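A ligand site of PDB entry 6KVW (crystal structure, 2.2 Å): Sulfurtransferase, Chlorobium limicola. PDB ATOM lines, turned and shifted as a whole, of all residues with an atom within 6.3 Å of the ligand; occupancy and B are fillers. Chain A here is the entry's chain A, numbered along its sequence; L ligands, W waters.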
ATOM      1  N   TYR A 191       6.161 -35.226  18.687  1.00  0.00           N
ATOM      2  CA  TYR A 191       5.447 -35.605  19.893  1.00  0.00           C
ATOM      3  C   TYR A 191       4.388 -36.653  19.535  1.00  0.00           C
ATOM      4  O   TYR A 191       3.366 -36.323  18.921  1.00  0.00           O
ATOM      5  CB  TYR A 191       4.812 -34.390  20.559  1.00  0.00           C
ATOM      6  CG  TYR A 191       3.868 -34.703  21.708  1.00  0.00           C
ATOM      7  CD1 TYR A 191       4.255 -35.559  22.736  1.00  0.00           C
ATOM      8  CD2 TYR A 191       2.603 -34.132  21.769  1.00  0.00           C
ATOM      9  CE1 TYR A 191       3.406 -35.843  23.783  1.00  0.00           C
ATOM     10  CE2 TYR A 191       1.743 -34.409  22.811  1.00  0.00           C
ATOM     11  CZ  TYR A 191       2.143 -35.263  23.813  1.00  0.00           C
ATOM     12  OH  TYR A 191       1.291 -35.543  24.851  1.00  0.00           O
ATOM     13  N   THR A 210       9.421 -36.833  21.564  1.00  0.00           N
ATOM     14  CA  THR A 210       9.728 -35.929  22.693  1.00  0.00           C
ATOM     15  C   THR A 210       9.515 -36.634  24.042  1.00  0.00           C
ATOM     16  O   THR A 210      10.179 -36.259  24.969  1.00  0.00           O
ATOM     17  CB  THR A 210       9.029 -34.577  22.571  1.00  0.00           C
ATOM     18  OG1 THR A 210       7.630 -34.767  22.566  1.00  0.00           O
ATOM     19  CG2 THR A 210       9.460 -33.800  21.343  1.00  0.00           C
ATOM     20  N   GLU A 214      11.365 -36.358  27.955  1.00  0.00           N
ATOM     21  CA  GLU A 214      10.558 -35.688  28.975  1.00  0.00           C
ATOM     22  C   GLU A 214       9.414 -36.599  29.406  1.00  0.00           C
ATOM     23  O   GLU A 214       8.854 -37.358  28.608  1.00  0.00           O
ATOM     24  CB  GLU A 214      10.013 -34.337  28.488  1.00  0.00           C
ATOM     25  CG  GLU A 214       9.052 -34.401  27.314  1.00  0.00           C
ATOM     26  CD  GLU A 214       8.580 -33.035  26.848  1.00  0.00           C
ATOM     27  OE1 GLU A 214       9.141 -32.020  27.309  1.00  0.00           O
ATOM     28  OE2 GLU A 214       7.653 -32.967  26.016  1.00  0.00           O
ATOM     29  N   TRP A 219       5.855 -33.378  32.663  1.00  0.00           N
ATOM     30  CA  TRP A 219       6.241 -32.634  31.466  1.00  0.00           C
ATOM     31  C   TRP A 219       7.542 -31.856  31.689  1.00  0.00           C
ATOM     32  O   TRP A 219       7.795 -30.847  31.025  1.00  0.00           O
ATOM     33  CB  TRP A 219       5.113 -31.716  30.971  1.00  0.00           C
ATOM     34  CG  TRP A 219       3.892 -32.491  30.527  1.00  0.00           C
ATOM     35  CD1 TRP A 219       2.619 -32.331  30.992  1.00  0.00           C
ATOM     36  CD2 TRP A 219       3.838 -33.537  29.552  1.00  0.00           C
ATOM     37  NE1 TRP A 219       1.772 -33.203  30.354  1.00  0.00           N
ATOM     38  CE2 TRP A 219       2.490 -33.963  29.474  1.00  0.00           C
ATOM     39  CE3 TRP A 219       4.783 -34.167  28.739  1.00  0.00           C
ATOM     40  CZ2 TRP A 219       2.079 -34.976  28.605  1.00  0.00           C
ATOM     41  CZ3 TRP A 219       4.368 -35.167  27.876  1.00  0.00           C
ATOM     42  CH2 TRP A 219       3.028 -35.569  27.819  1.00  0.00           C
ATOM     43  N   PHE A 257      -4.065 -33.735  20.547  1.00  0.00           N
ATOM     44  CA  PHE A 257      -2.642 -33.490  20.750  1.00  0.00           C
ATOM     45  C   PHE A 257      -2.146 -32.544  19.659  1.00  0.00           C
ATOM     46  O   PHE A 257      -1.510 -32.968  18.691  1.00  0.00           O
ATOM     47  CB  PHE A 257      -1.849 -34.801  20.731  1.00  0.00           C
ATOM     48  CG  PHE A 257      -2.324 -35.794  21.751  1.00  0.00           C
ATOM     49  CD1 PHE A 257      -2.185 -35.549  23.103  1.00  0.00           C
ATOM     50  CD2 PHE A 257      -2.908 -36.988  21.340  1.00  0.00           C
ATOM     51  CE1 PHE A 257      -2.619 -36.469  24.044  1.00  0.00           C
ATOM     52  CE2 PHE A 257      -3.338 -37.919  22.275  1.00  0.00           C
ATOM     53  CZ  PHE A 257      -3.192 -37.653  23.624  1.00  0.00           C
ATOM     54  N   PRO A 258      -2.432 -31.238  19.792  1.00  0.00           N
ATOM     55  CA  PRO A 258      -1.926 -30.280  18.794  1.00  0.00           C
ATOM     56  C   PRO A 258      -0.403 -30.218  18.744  1.00  0.00           C
ATOM     57  O   PRO A 258       0.145 -29.809  17.717  1.00  0.00           O
ATOM     58  CB  PRO A 258      -2.526 -28.945  19.245  1.00  0.00           C
ATOM     59  CG  PRO A 258      -3.688 -29.322  20.130  1.00  0.00           C
ATOM     60  CD  PRO A 258      -3.274 -30.596  20.809  1.00  0.00           C
ATOM     61  N   GLY A 259       0.275 -30.629  19.814  1.00  0.00           N
ATOM     62  CA  GLY A 259       1.726 -30.644  19.828  1.00  0.00           C
ATOM     63  C   GLY A 259       2.342 -31.594  18.824  1.00  0.00           C
ATOM     64  O   GLY A 259       3.498 -31.412  18.427  1.00  0.00           O
ATOM     65  N   SER A 260       1.588 -32.614  18.399  1.00  0.00           N
ATOM     66  CA  SER A 260       2.065 -33.531  17.366  1.00  0.00           C
ATOM     67  C   SER A 260       2.307 -32.836  16.039  1.00  0.00           C
ATOM     68  O   SER A 260       2.995 -33.386  15.170  1.00  0.00           O
ATOM     69  CB  SER A 260       1.078 -34.683  17.190  1.00  0.00           C
ATOM     70  OG  SER A 260       0.948 -35.437  18.373  1.00  0.00           O
ATOM     71  N   ALA A 262       3.372 -29.413  15.985  1.00  0.00           N
ATOM     72  CA  ALA A 262       4.368 -28.370  16.200  1.00  0.00           C
ATOM     73  C   ALA A 262       5.747 -29.007  16.385  1.00  0.00           C
ATOM     74  O   ALA A 262       6.373 -28.931  17.436  1.00  0.00           O
ATOM     75  CB  ALA A 262       3.970 -27.509  17.390  1.00  0.00           C
ATOM     76  N   ILE A 265       9.103 -26.754  17.325  1.00  0.00           N
ATOM     77  CA  ILE A 265       9.203 -26.365  18.728  1.00  0.00           C
ATOM     78  C   ILE A 265       9.734 -27.522  19.552  1.00  0.00           C
ATOM     79  O   ILE A 265      10.620 -27.353  20.399  1.00  0.00           O
ATOM     80  CB  ILE A 265       7.849 -25.873  19.272  1.00  0.00           C
ATOM     81  CG1 ILE A 265       7.240 -24.804  18.372  1.00  0.00           C
ATOM     82  CG2 ILE A 265       8.021 -25.339  20.687  1.00  0.00           C
ATOM     83  CD1 ILE A 265       5.931 -24.255  18.918  1.00  0.00           C
ATOM     84  N   TYR A 356      -4.070 -25.269  27.182  1.00  0.00           N
ATOM     85  CA  TYR A 356      -3.910 -26.693  26.995  1.00  0.00           C
ATOM     86  C   TYR A 356      -5.180 -27.402  27.435  1.00  0.00           C
ATOM     87  O   TYR A 356      -5.873 -26.942  28.344  1.00  0.00           O
ATOM     88  CB  TYR A 356      -2.718 -27.238  27.796  1.00  0.00           C
ATOM     89  CG  TYR A 356      -1.413 -26.502  27.549  1.00  0.00           C
ATOM     90  CD1 TYR A 356      -1.122 -25.324  28.231  1.00  0.00           C
ATOM     91  CD2 TYR A 356      -0.482 -26.982  26.649  1.00  0.00           C
ATOM     92  CE1 TYR A 356       0.065 -24.652  28.009  1.00  0.00           C
ATOM     93  CE2 TYR A 356       0.707 -26.318  26.412  1.00  0.00           C
ATOM     94  CZ  TYR A 356       0.974 -25.153  27.105  1.00  0.00           C
ATOM     95  OH  TYR A 356       2.159 -24.498  26.865  1.00  0.00           O
ATOM     96  N   TYR A 358      -5.233 -30.208  28.906  1.00  0.00           N
ATOM     97  CA  TYR A 358      -4.931 -30.989  30.100  1.00  0.00           C
ATOM     98  C   TYR A 358      -4.580 -30.106  31.298  1.00  0.00           C
ATOM     99  O   TYR A 358      -4.092 -30.624  32.314  1.00  0.00           O
ATOM    100  CB  TYR A 358      -3.800 -31.974  29.824  1.00  0.00           C
ATOM    101  CG  TYR A 358      -2.548 -31.344  29.252  1.00  0.00           C
ATOM    102  CD1 TYR A 358      -1.534 -30.872  30.076  1.00  0.00           C
ATOM    103  CD2 TYR A 358      -2.375 -31.229  27.878  1.00  0.00           C
ATOM    104  CE1 TYR A 358      -0.394 -30.293  29.556  1.00  0.00           C
ATOM    105  CE2 TYR A 358      -1.233 -30.658  27.342  1.00  0.00           C
ATOM    106  CZ  TYR A 358      -0.244 -30.192  28.192  1.00  0.00           C
ATOM    107  OH  TYR A 358       0.884 -29.627  27.657  1.00  0.00           O
ATOM    108  N   ALA A 377      -0.706 -21.832  22.288  1.00  0.00           N
ATOM    109  CA  ALA A 377       0.426 -22.562  22.842  1.00  0.00           C
ATOM    110  C   ALA A 377       1.238 -23.305  21.789  1.00  0.00           C
ATOM    111  O   ALA A 377       2.344 -23.750  22.106  1.00  0.00           O
ATOM    112  CB  ALA A 377      -0.057 -23.544  23.914  1.00  0.00           C
ATOM    113  N   TYR A 378       0.741 -23.431  20.570  1.00  0.00           N
ATOM    114  CA  TYR A 378       1.387 -24.251  19.548  1.00  0.00           C
ATOM    115  C   TYR A 378       1.888 -23.431  18.367  1.00  0.00           C
ATOM    116  O   TYR A 378       2.156 -23.985  17.301  1.00  0.00           O
ATOM    117  CB  TYR A 378       0.427 -25.355  19.094  1.00  0.00           C
ATOM    118  CG  TYR A 378      -0.048 -26.205  20.256  1.00  0.00           C
ATOM    119  CD1 TYR A 378       0.716 -27.274  20.711  1.00  0.00           C
ATOM    120  CD2 TYR A 378      -1.243 -25.920  20.902  1.00  0.00           C
ATOM    121  CE1 TYR A 378       0.298 -28.041  21.771  1.00  0.00           C
ATOM    122  CE2 TYR A 378      -1.671 -26.696  21.972  1.00  0.00           C
ATOM    123  CZ  TYR A 378      -0.892 -27.751  22.395  1.00  0.00           C
ATOM    124  OH  TYR A 378      -1.298 -28.525  23.461  1.00  0.00           O
ATOM    125  N   HIS A 379       2.048 -22.122  18.544  1.00  0.00           N
ATOM    126  CA  HIS A 379       2.577 -21.227  17.523  1.00  0.00           C
ATOM    127  C   HIS A 379       3.481 -20.190  18.175  1.00  0.00           C
ATOM    128  O   HIS A 379       3.229 -19.758  19.306  1.00  0.00           O
ATOM    129  CB  HIS A 379       1.462 -20.528  16.737  1.00  0.00           C
ATOM    130  CG  HIS A 379       0.536 -21.464  16.023  1.00  0.00           C
ATOM    131  ND1 HIS A 379      -0.540 -22.070  16.638  1.00  0.00           N
ATOM    132  CD2 HIS A 379       0.535 -21.905  14.739  1.00  0.00           C
ATOM    133  CE1 HIS A 379      -1.162 -22.843  15.760  1.00  0.00           C
ATOM    134  NE2 HIS A 379      -0.534 -22.750  14.607  1.00  0.00           N
ATOM    135  N   CSS A 415       6.913 -21.440  29.856  1.00  0.00           N
ATOM    136  CA  CSS A 415       5.606 -21.329  29.254  1.00  0.00           C
ATOM    137  CB  CSS A 415       5.646 -21.668  27.757  1.00  0.00           C
ATOM    138  SG  CSS A 415       6.560 -23.147  27.442  1.00  0.00           S
ATOM    139  SD  CSS A 415       5.132 -24.406  26.759  1.00  0.00           S
ATOM    140  C   CSS A 415       4.673 -22.246  29.998  1.00  0.00           C
ATOM    141  O   CSS A 415       4.761 -22.313  31.237  1.00  0.00           O
ATOM    142  N   GLY A 416       3.950 -23.082  29.264  1.00  0.00           N
ATOM    143  CA  GLY A 416       3.078 -24.060  29.877  1.00  0.00           C
ATOM    144  C   GLY A 416       3.850 -25.239  30.449  1.00  0.00           C
ATOM    145  O   GLY A 416       3.718 -25.551  31.637  1.00  0.00           O
ATOM    146  N   THR A 417       4.653 -25.882  29.611  1.00  0.00           N
ATOM    147  CA  THR A 417       5.447 -27.035  30.021  1.00  0.00           C
ATOM    148  C   THR A 417       6.919 -26.923  29.669  1.00  0.00           C
ATOM    149  O   THR A 417       7.691 -27.819  30.041  1.00  0.00           O
ATOM    150  CB  THR A 417       4.881 -28.328  29.416  1.00  0.00           C
ATOM    151  OG1 THR A 417       5.014 -28.295  27.993  1.00  0.00           O
ATOM    152  CG2 THR A 417       3.416 -28.509  29.791  1.00  0.00           C
ATOM    153  N   GLY A 418       7.345 -25.878  28.977  1.00  0.00           N
ATOM    154  CA  GLY A 418       8.745 -25.675  28.673  1.00  0.00           C
ATOM    155  C   GLY A 418       9.109 -25.731  27.196  1.00  0.00           C
ATOM    156  O   GLY A 418      10.279 -25.495  26.865  1.00  0.00           O
ATOM    157  N   TRP A 419       8.174 -26.056  26.293  1.00  0.00           N
ATOM    158  CA  TRP A 419       8.497 -26.075  24.877  1.00  0.00           C
ATOM    159  C   TRP A 419       8.795 -24.678  24.350  1.00  0.00           C
ATOM    160  O   TRP A 419       9.869 -24.417  23.797  1.00  0.00           O
ATOM    161  CB  TRP A 419       7.352 -26.711  24.082  1.00  0.00           C
ATOM    162  CG  TRP A 419       7.401 -28.194  24.010  1.00  0.00           C
ATOM    163  CD1 TRP A 419       7.827 -29.062  24.977  1.00  0.00           C
ATOM    164  CD2 TRP A 419       7.029 -29.009  22.892  1.00  0.00           C
ATOM    165  NE1 TRP A 419       7.724 -30.356  24.545  1.00  0.00           N
ATOM    166  CE2 TRP A 419       7.240 -30.353  23.267  1.00  0.00           C
ATOM    167  CE3 TRP A 419       6.511 -28.735  21.620  1.00  0.00           C
ATOM    168  CZ2 TRP A 419       6.964 -31.415  22.409  1.00  0.00           C
ATOM    169  CZ3 TRP A 419       6.243 -29.792  20.773  1.00  0.00           C
ATOM    170  CH2 TRP A 419       6.465 -31.122  21.161  1.00  0.00           C
ATOM    171  N   ARG A 420       7.848 -23.754  24.519  1.00  0.00           N
ATOM    172  CA  ARG A 420       8.035 -22.400  24.013  1.00  0.00           C
ATOM    173  C   ARG A 420       9.134 -21.674  24.781  1.00  0.00           C
ATOM    174  O   ARG A 420       9.902 -20.907  24.192  1.00  0.00           O
ATOM    175  CB  ARG A 420       6.723 -21.631  24.083  1.00  0.00           C
ATOM    176  CG  ARG A 420       5.642 -22.199  23.189  1.00  0.00           C
ATOM    177  CD  ARG A 420       4.330 -21.492  23.423  1.00  0.00           C
ATOM    178  NE  ARG A 420       3.760 -21.856  24.712  1.00  0.00           N
ATOM    179  CZ  ARG A 420       2.713 -21.254  25.258  1.00  0.00           C
ATOM    180  NH1 ARG A 420       2.128 -20.246  24.629  1.00  0.00           N
ATOM    181  NH2 ARG A 420       2.263 -21.647  26.446  1.00  0.00           N
HETATM  182  C1  LIG L   1       4.582 -31.431  26.787  1.00  0.00           C
HETATM  183  C2  LIG L   1       4.208 -32.402  24.557  1.00  0.00           C
HETATM  184  C3  LIG L   1       2.368 -32.404  26.219  1.00  0.00           C
HETATM  185  O1  LIG L   1       0.782 -29.772  24.868  1.00  0.00           O
HETATM  186  O2  LIG L   1       1.866 -30.817  23.208  1.00  0.00           O
HETATM  187  C4  LIG L   1       3.607 -27.563  22.838  1.00  0.00           C
HETATM  188  C5  LIG L   1       4.212 -29.491  24.448  1.00  0.00           C
HETATM  189  N1  LIG L   1       3.857 -27.016  24.913  1.00  0.00           N
HETATM  190  N2  LIG L   1       3.386 -26.181  22.921  1.00  0.00           N
HETATM  191  C6  LIG L   1       1.775 -30.301  24.290  1.00  0.00           C
HETATM  192  C7  LIG L   1       3.903 -28.074  24.075  1.00  0.00           C
HETATM  193  C8  LIG L   1       3.549 -25.848  24.250  1.00  0.00           C
HETATM  194  C9  LIG L   1       3.098 -30.175  25.230  1.00  0.00           C
HETATM  195  N3  LIG L   1       3.548 -31.600  25.698  1.00  0.00           N
HETATM  196  O   HOH W   1       7.280 -30.226  28.366  1.00  0.00           O
HETATM  197  O   HOH W   2      -0.622 -33.728  25.549  1.00  0.00           O
HETATM  198  O   HOH W   3      -0.422 -31.672  22.307  1.00  0.00           O
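Merely in contact with the ligand: Trp 419 (3.3 Å), Tyr 356 (3.3 Å), Trp 219 (3.4 Å), Gly 259 (3.4 Å), Thr 417 (3.4 Å), Glu 214 (3.5 Å) and Tyr 191 (3.6 Å).
Hydrophobic or aromatic side chains that line the ligand: Tyr 191, Trp 219, Tyr 356, Tyr 358, Tyr 378 and Trp 419.
11 residues have an atom within 4 Å of the ligand: Tyr 191, Glu 214, Trp 219, Gly 259, Tyr 356, Tyr 358, Ala 377, Tyr 378, CSS 415, Thr 417 and Trp 419.
The nearest printed residue that does not touch the ligand is Arg 420 (4.02 Å).
The side-chain hydroxyl (OH) of Tyr 358 is in hydrogen-bond range of an oxygen (O1) of the ligand, at 2.8 Å.
The backbone carbonyl oxygen of Ala 377 lies close to a nitrogen (N2) of the ligand.
SD of CSS 415 lies close to N1 of the ligand, at 3.4 Å.
OH of Tyr 378 is in hydrogen-bond range of O1 of the ligand, 2.8 Å away.
SG of CSS 415 sits at hydrogen-bond distance from N of Gly 418, at 3.2 Å.
The side-chain hydroxyl (OH) of Tyr 356 lies within hydrogen-bond range of the guanidinium group (NH2) of Arg 420 (2.9 Å).
N of Trp 419 lies within hydrogen-bond range of SD of CSS 415 (3.5 Å).
OH of Tyr 356 sits at hydrogen-bond distance from SD of CSS 415 (3.0 Å).
NE1 of Trp 419 lies within hydrogen-bond range of OE2 of Glu 214 (3.0 Å).
SD of CSS 415 lies within hydrogen-bond range of the backbone NH (N) of Thr 417.
O of Tyr 191 lies within hydrogen-bond range of OG of Ser 260 (2.6 Å).
The side-chain hydroxyl (OH) of Tyr 356 sits close to the backbone NH (N) of Gly 416.
Water W3 lies within hydrogen-bond range of O2 of the ligand (2.6 Å), N of Gly 259 (2.8 Å) and OH of Tyr 378 (3.5 Å).
Water W1 lies within hydrogen-bond range of OE1 of Glu 214 and OG1 of Thr 417.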
